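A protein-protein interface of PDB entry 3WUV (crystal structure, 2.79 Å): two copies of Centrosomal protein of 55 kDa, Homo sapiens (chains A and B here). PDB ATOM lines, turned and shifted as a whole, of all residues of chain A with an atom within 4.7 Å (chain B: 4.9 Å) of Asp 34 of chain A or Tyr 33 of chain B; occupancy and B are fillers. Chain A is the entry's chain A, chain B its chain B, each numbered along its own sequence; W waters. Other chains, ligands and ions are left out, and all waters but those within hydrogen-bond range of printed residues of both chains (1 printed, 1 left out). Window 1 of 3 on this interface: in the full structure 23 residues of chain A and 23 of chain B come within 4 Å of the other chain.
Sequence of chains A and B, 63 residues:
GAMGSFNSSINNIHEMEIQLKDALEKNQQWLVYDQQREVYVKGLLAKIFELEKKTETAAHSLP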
ATOM      1  N   TRP A  30      -3.154  10.479 -10.186  1.00  0.00           N
ATOM      2  CA  TRP A  30      -2.941   9.532 -11.274  1.00  0.00           C
ATOM      3  C   TRP A  30      -1.665   9.834 -12.046  1.00  0.00           C
ATOM      4  O   TRP A  30      -0.940   8.920 -12.438  1.00  0.00           O
ATOM      5  CB  TRP A  30      -4.130   9.534 -12.236  1.00  0.00           C
ATOM      6  CG  TRP A  30      -5.208   8.577 -11.855  1.00  0.00           C
ATOM      7  CD1 TRP A  30      -6.471   8.885 -11.444  1.00  0.00           C
ATOM      8  CD2 TRP A  30      -5.118   7.150 -11.847  1.00  0.00           C
ATOM      9  NE1 TRP A  30      -7.176   7.734 -11.184  1.00  0.00           N
ATOM     10  CE2 TRP A  30      -6.367   6.655 -11.422  1.00  0.00           C
ATOM     11  CE3 TRP A  30      -4.102   6.241 -12.158  1.00  0.00           C
ATOM     12  CZ2 TRP A  30      -6.627   5.293 -11.301  1.00  0.00           C
ATOM     13  CZ3 TRP A  30      -4.362   4.890 -12.038  1.00  0.00           C
ATOM     14  CH2 TRP A  30      -5.614   4.428 -11.613  1.00  0.00           C
ATOM     15  N   LEU A  31      -1.397  11.117 -12.265  1.00  0.00           N
ATOM     16  CA  LEU A  31      -0.208  11.529 -12.998  1.00  0.00           C
ATOM     17  C   LEU A  31       1.063  11.064 -12.296  1.00  0.00           C
ATOM     18  O   LEU A  31       1.938  10.463 -12.917  1.00  0.00           O
ATOM     19  CB  LEU A  31      -0.181  13.047 -13.179  1.00  0.00           C
ATOM     20  CG  LEU A  31       1.018  13.574 -13.967  1.00  0.00           C
ATOM     21  CD1 LEU A  31       1.061  12.944 -15.349  1.00  0.00           C
ATOM     22  CD2 LEU A  31       0.978  15.087 -14.069  1.00  0.00           C
ATOM     23  N   VAL A  32       1.155  11.340 -10.998  1.00  0.00           N
ATOM     24  CA  VAL A  32       2.309  10.939 -10.203  1.00  0.00           C
ATOM     25  C   VAL A  32       2.405   9.418 -10.114  1.00  0.00           C
ATOM     26  O   VAL A  32       3.472   8.839 -10.326  1.00  0.00           O
ATOM     27  CB  VAL A  32       2.243  11.531  -8.781  1.00  0.00           C
ATOM     28  CG1 VAL A  32       3.376  10.987  -7.924  1.00  0.00           C
ATOM     29  CG2 VAL A  32       2.289  13.051  -8.835  1.00  0.00           C
ATOM     30  N   TYR A  33       1.278   8.786  -9.799  1.00  0.00           N
ATOM     31  CA  TYR A  33       1.172   7.331  -9.745  1.00  0.00           C
ATOM     32  C   TYR A  33       1.661   6.701 -11.045  1.00  0.00           C
ATOM     33  O   TYR A  33       2.315   5.660 -11.028  1.00  0.00           O
ATOM     34  CB  TYR A  33      -0.282   6.932  -9.475  1.00  0.00           C
ATOM     35  CG  TYR A  33      -0.564   5.444  -9.412  1.00  0.00           C
ATOM     36  CD1 TYR A  33      -0.493   4.752  -8.210  1.00  0.00           C
ATOM     37  CD2 TYR A  33      -0.938   4.739 -10.549  1.00  0.00           C
ATOM     38  CE1 TYR A  33      -0.768   3.396  -8.148  1.00  0.00           C
ATOM     39  CE2 TYR A  33      -1.213   3.386 -10.496  1.00  0.00           C
ATOM     40  CZ  TYR A  33      -1.127   2.720  -9.295  1.00  0.00           C
ATOM     41  OH  TYR A  33      -1.401   1.372  -9.243  1.00  0.00           O
ATOM     42  N   ASP A  34       1.349   7.343 -12.169  1.00  0.00           N
ATOM     43  CA  ASP A  34       1.750   6.841 -13.480  1.00  0.00           C
ATOM     44  C   ASP A  34       3.228   7.085 -13.760  1.00  0.00           C
ATOM     45  O   ASP A  34       3.902   6.235 -14.342  1.00  0.00           O
ATOM     46  CB  ASP A  34       0.906   7.477 -14.586  1.00  0.00           C
ATOM     47  CG  ASP A  34       1.097   6.795 -15.929  1.00  0.00           C
ATOM     48  OD1 ASP A  34       0.946   5.556 -15.990  1.00  0.00           O
ATOM     49  OD2 ASP A  34       1.411   7.493 -16.919  1.00  0.00           O
ATOM     50  N   GLN A  35       3.725   8.252 -13.356  1.00  0.00           N
ATOM     51  CA  GLN A  35       5.134   8.583 -13.538  1.00  0.00           C
ATOM     52  C   GLN A  35       6.023   7.553 -12.853  1.00  0.00           C
ATOM     53  O   GLN A  35       7.065   7.168 -13.382  1.00  0.00           O
ATOM     54  CB  GLN A  35       5.441   9.982 -13.000  1.00  0.00           C
ATOM     55  CG  GLN A  35       4.844  11.109 -13.819  1.00  0.00           C
ATOM     56  CD  GLN A  35       5.202  12.477 -13.274  1.00  0.00           C
ATOM     57  OE1 GLN A  35       4.714  12.885 -12.219  1.00  0.00           O
ATOM     58  NE2 GLN A  35       6.064  13.191 -13.988  1.00  0.00           N
ATOM     59  N   GLN A  36       5.597   7.102 -11.677  1.00  0.00           N
ATOM     60  CA  GLN A  36       6.343   6.098 -10.929  1.00  0.00           C
ATOM     61  C   GLN A  36       6.298   4.738 -11.622  1.00  0.00           C
ATOM     62  O   GLN A  36       7.297   4.019 -11.647  1.00  0.00           O
ATOM     63  CB  GLN A  36       5.823   6.002  -9.494  1.00  0.00           C
ATOM     64  CG  GLN A  36       6.006   7.286  -8.697  1.00  0.00           C
ATOM     65  CD  GLN A  36       5.288   7.268  -7.361  1.00  0.00           C
ATOM     66  OE1 GLN A  36       4.675   6.269  -6.983  1.00  0.00           O
ATOM     67  NE2 GLN A  36       5.357   8.382  -6.640  1.00  0.00           N
ATOM     68  N   ARG A  37       5.148   4.390 -12.193  1.00  0.00           N
ATOM     69  CA  ARG A  37       5.031   3.142 -12.943  1.00  0.00           C
ATOM     70  C   ARG A  37       5.939   3.169 -14.169  1.00  0.00           C
ATOM     71  O   ARG A  37       6.455   2.137 -14.598  1.00  0.00           O
ATOM     72  CB  ARG A  37       3.580   2.875 -13.352  1.00  0.00           C
ATOM     73  CG  ARG A  37       3.408   1.673 -14.271  1.00  0.00           C
ATOM     74  CD  ARG A  37       1.957   1.244 -14.357  1.00  0.00           C
ATOM     75  NE  ARG A  37       1.080   2.361 -14.688  1.00  0.00           N
ATOM     76  CZ  ARG A  37      -0.240   2.342 -14.531  1.00  0.00           C
ATOM     77  NH1 ARG A  37      -0.838   1.264 -14.043  1.00  0.00           N
ATOM     78  NH2 ARG A  37      -0.960   3.405 -14.854  1.00  0.00           N
ATOM     79  N   GLU A  38       6.144   4.358 -14.721  1.00  0.00           N
ATOM     80  CA  GLU A  38       7.040   4.518 -15.858  1.00  0.00           C
ATOM     81  C   GLU A  38       8.493   4.286 -15.449  1.00  0.00           C
ATOM     82  O   GLU A  38       9.272   3.707 -16.206  1.00  0.00           O
ATOM     83  CB  GLU A  38       6.862   5.894 -16.505  1.00  0.00           C
ATOM     84  CG  GLU A  38       5.605   6.011 -17.353  1.00  0.00           C
ATOM     85  CD  GLU A  38       5.574   5.006 -18.495  1.00  0.00           C
ATOM     86  OE1 GLU A  38       6.565   4.932 -19.254  1.00  0.00           O
ATOM     87  OE2 GLU A  38       4.562   4.284 -18.625  1.00  0.00           O
ATOM     88  N   GLN B  29     -10.394   8.681 -18.651  1.00  0.00           N
ATOM     89  CA  GLN B  29      -9.267   8.287 -19.492  1.00  0.00           C
ATOM     90  C   GLN B  29      -8.140   7.653 -18.684  1.00  0.00           C
ATOM     91  O   GLN B  29      -7.478   6.730 -19.153  1.00  0.00           O
ATOM     92  CB  GLN B  29      -8.735   9.475 -20.298  1.00  0.00           C
ATOM     93  CG  GLN B  29      -9.676   9.933 -21.391  1.00  0.00           C
ATOM     94  CD  GLN B  29     -10.181   8.779 -22.227  1.00  0.00           C
ATOM     95  OE1 GLN B  29      -9.435   8.189 -23.005  1.00  0.00           O
ATOM     96  NE2 GLN B  29     -11.453   8.439 -22.059  1.00  0.00           N
ATOM     97  N   TRP B  30      -7.928   8.153 -17.470  1.00  0.00           N
ATOM     98  CA  TRP B  30      -6.920   7.588 -16.580  1.00  0.00           C
ATOM     99  C   TRP B  30      -7.232   6.135 -16.241  1.00  0.00           C
ATOM    100  O   TRP B  30      -6.346   5.281 -16.245  1.00  0.00           O
ATOM    101  CB  TRP B  30      -6.803   8.419 -15.298  1.00  0.00           C
ATOM    102  CG  TRP B  30      -6.002   9.670 -15.473  1.00  0.00           C
ATOM    103  CD1 TRP B  30      -6.455  10.955 -15.407  1.00  0.00           C
ATOM    104  CD2 TRP B  30      -4.600   9.752 -15.754  1.00  0.00           C
ATOM    105  NE1 TRP B  30      -5.420  11.833 -15.625  1.00  0.00           N
ATOM    106  CE2 TRP B  30      -4.271  11.119 -15.842  1.00  0.00           C
ATOM    107  CE3 TRP B  30      -3.591   8.802 -15.939  1.00  0.00           C
ATOM    108  CZ2 TRP B  30      -2.976  11.559 -16.108  1.00  0.00           C
ATOM    109  CZ3 TRP B  30      -2.307   9.241 -16.202  1.00  0.00           C
ATOM    110  CH2 TRP B  30      -2.011  10.607 -16.283  1.00  0.00           C
ATOM    111  N   LEU B  31      -8.502   5.865 -15.960  1.00  0.00           N
ATOM    112  CA  LEU B  31      -8.952   4.529 -15.580  1.00  0.00           C
ATOM    113  C   LEU B  31      -8.703   3.479 -16.666  1.00  0.00           C
ATOM    114  O   LEU B  31      -8.275   2.364 -16.367  1.00  0.00           O
ATOM    115  CB  LEU B  31     -10.434   4.560 -15.190  1.00  0.00           C
ATOM    116  CG  LEU B  31     -10.778   4.786 -13.713  1.00  0.00           C
ATOM    117  CD1 LEU B  31     -10.116   6.035 -13.158  1.00  0.00           C
ATOM    118  CD2 LEU B  31     -12.286   4.856 -13.521  1.00  0.00           C
ATOM    119  N   VAL B  32      -8.974   3.828 -17.921  1.00  0.00           N
ATOM    120  CA  VAL B  32      -8.694   2.921 -19.031  1.00  0.00           C
ATOM    121  C   VAL B  32      -7.187   2.804 -19.273  1.00  0.00           C
ATOM    122  O   VAL B  32      -6.673   1.715 -19.537  1.00  0.00           O
ATOM    123  CB  VAL B  32      -9.441   3.331 -20.332  1.00  0.00           C
ATOM    124  CG1 VAL B  32      -9.822   4.788 -20.294  1.00  0.00           C
ATOM    125  CG2 VAL B  32      -8.606   3.027 -21.571  1.00  0.00           C
ATOM    126  N   TYR B  33      -6.484   3.929 -19.159  1.00  0.00           N
ATOM    127  CA  TYR B  33      -5.033   3.955 -19.327  1.00  0.00           C
ATOM    128  C   TYR B  33      -4.334   3.085 -18.284  1.00  0.00           C
ATOM    129  O   TYR B  33      -3.360   2.396 -18.588  1.00  0.00           O
ATOM    130  CB  TYR B  33      -4.511   5.390 -19.242  1.00  0.00           C
ATOM    131  CG  TYR B  33      -3.031   5.528 -19.529  1.00  0.00           C
ATOM    132  CD1 TYR B  33      -2.547   5.456 -20.828  1.00  0.00           C
ATOM    133  CD2 TYR B  33      -2.120   5.743 -18.504  1.00  0.00           C
ATOM    134  CE1 TYR B  33      -1.198   5.586 -21.100  1.00  0.00           C
ATOM    135  CE2 TYR B  33      -0.764   5.876 -18.766  1.00  0.00           C
ATOM    136  CZ  TYR B  33      -0.310   5.795 -20.068  1.00  0.00           C
ATOM    137  OH  TYR B  33       1.035   5.924 -20.338  1.00  0.00           O
ATOM    138  N   ASP B  34      -4.838   3.130 -17.054  1.00  0.00           N
ATOM    139  CA  ASP B  34      -4.307   2.317 -15.965  1.00  0.00           C
ATOM    140  C   ASP B  34      -4.420   0.838 -16.307  1.00  0.00           C
ATOM    141  O   ASP B  34      -3.480   0.066 -16.121  1.00  0.00           O
ATOM    142  CB  ASP B  34      -5.071   2.607 -14.673  1.00  0.00           C
ATOM    143  CG  ASP B  34      -4.675   1.682 -13.541  1.00  0.00           C
ATOM    144  OD1 ASP B  34      -3.598   1.900 -12.946  1.00  0.00           O
ATOM    145  OD2 ASP B  34      -5.440   0.740 -13.243  1.00  0.00           O
ATOM    146  N   GLN B  35      -5.589   0.467 -16.813  1.00  0.00           N
ATOM    147  CA  GLN B  35      -5.897  -0.905 -17.190  1.00  0.00           C
ATOM    148  C   GLN B  35      -4.980  -1.392 -18.305  1.00  0.00           C
ATOM    149  O   GLN B  35      -4.580  -2.556 -18.332  1.00  0.00           O
ATOM    150  CB  GLN B  35      -7.352  -0.978 -17.648  1.00  0.00           C
ATOM    151  CG  GLN B  35      -7.888  -2.370 -17.877  1.00  0.00           C
ATOM    152  CD  GLN B  35      -9.303  -2.350 -18.426  1.00  0.00           C
ATOM    153  OE1 GLN B  35      -9.926  -1.292 -18.530  1.00  0.00           O
ATOM    154  NE2 GLN B  35      -9.815  -3.522 -18.786  1.00  0.00           N
ATOM    155  N   GLN B  36      -4.652  -0.495 -19.229  1.00  0.00           N
ATOM    156  CA  GLN B  36      -3.795  -0.848 -20.352  1.00  0.00           C
ATOM    157  C   GLN B  36      -2.331  -0.948 -19.929  1.00  0.00           C
ATOM    158  O   GLN B  36      -1.597  -1.802 -20.424  1.00  0.00           O
ATOM    159  CB  GLN B  36      -3.955   0.151 -21.503  1.00  0.00           C
ATOM    160  CG  GLN B  36      -5.309   0.094 -22.199  1.00  0.00           C
ATOM    161  CD  GLN B  36      -5.597  -1.265 -22.813  1.00  0.00           C
ATOM    162  OE1 GLN B  36      -6.277  -2.097 -22.213  1.00  0.00           O
ATOM    163  NE2 GLN B  36      -5.081  -1.494 -24.018  1.00  0.00           N
ATOM    164  N   ARG B  37      -1.908  -0.081 -19.013  1.00  0.00           N
ATOM    165  CA  ARG B  37      -0.513  -0.080 -18.571  1.00  0.00           C
ATOM    166  C   ARG B  37      -0.170  -1.280 -17.692  1.00  0.00           C
ATOM    167  O   ARG B  37       0.943  -1.798 -17.756  1.00  0.00           O
ATOM    168  CB  ARG B  37      -0.151   1.225 -17.856  1.00  0.00           C
ATOM    169  CG  ARG B  37      -0.085   2.431 -18.776  1.00  0.00           C
ATOM    170  CD  ARG B  37       0.684   2.117 -20.052  1.00  0.00           C
ATOM    171  NE  ARG B  37       2.121   2.355 -19.930  1.00  0.00           N
ATOM    172  CZ  ARG B  37       3.010   2.049 -20.871  1.00  0.00           C
ATOM    173  NH1 ARG B  37       2.611   1.482 -22.002  1.00  0.00           N
ATOM    174  NH2 ARG B  37       4.298   2.303 -20.681  1.00  0.00           N
HETATM  175  O   HOH W   1      -2.813  -0.036 -10.630  1.00  0.00           O
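The guanidinium group (NH1) of Arg 37 of chain A is in salt-bridge range of the side-chain carboxylate (OD1) of Asp 34 of chain B (3.0 Å). The side-chain carboxylate of Glu 38 of chain A lies within salt-bridge range of the guanidinium group of Arg 37 of chain B.
NH2 of Arg 37 of chain A is in salt-bridge range of OD1 of Asp 34 of chain A, at 3.1 Å.
CD2 of Trp 30 of chain B touches CB of Trp 30 of chain A (3.6 Å). Leu 31 of chain B touches Trp 30 of chain A (CD1 to NE1, 3.9 Å). CZ3 of Trp 30 of chain A touches OD1 of Asp 34 of chain B, at 3.2 Å. Trp 30 of chain B touches Leu 31 of chain A. OD1 of Asp 34 of chain B touches CE2 of Tyr 33 of chain A, 3.7 Å away. Asp 34 of chain A touches Tyr 33 of chain B (OD1 to CE2, 3.3 Å). CZ of Arg 37 of chain A touches CB of Arg 37 of chain B, 3.5 Å away.
Printed residues of chain B within 4 Å of Tyr 33 of chain A: Asp 34 (3.7 Å). Of the printed residues of chain B, Asp 34 of chain A touches Tyr 33. Printed residues of chain B within 4 Å of Arg 37 of chain A: Asp 34 and Arg 37. Of the printed residues of chain A, Trp 30 of chain B touches Trp 30 (3.6 Å) and Leu 31 (3.9 Å). Tyr 33 of chain B touches one residue of chain A. Gln 35 of chain B touches none of the printed residues of chain A. The nearest printed residue of chain B that does not touch Asp 34 of chain A is Trp 30 of chain B (4.01 Å).
Of the 9 printed residues of chain B, 5 touch a printed residue of chain A. Printed residues of chain B that touch a printed residue of chain A: Trp 30, Leu 31, Tyr 33, Asp 34 and Arg 37. Hydrophobic or aromatic side chains of chain B that line the printed part of chain A: Trp 30, Leu 31 and Tyr 33.
Trp 30 of chain A touches its own counterpart, Trp 30 of chain B. Trp 30 of chain A touches Asp 34 of chain B, but with the chains exchanged Asp 34 of chain A does not touch Trp 30 of chain B (4.01 Å). Tyr 33 of chain A touches Asp 34 of chain B, and with the chains exchanged Asp 34 of chain A touches Tyr 33 of chain B. Arg 37 of chain A touches Asp 34 of chain B, but with the chains exchanged Asp 34 of chain A does not touch Arg 37 of chain B (4.3 Å). Positions printed for both chains: 30, 31, 32, 33, 34, 35, 36 and 37.
Water W1 bridges OH of Tyr 33 of chain A (2.4 Å) and OD1 of Asp 34 of chain B (3.1 Å).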
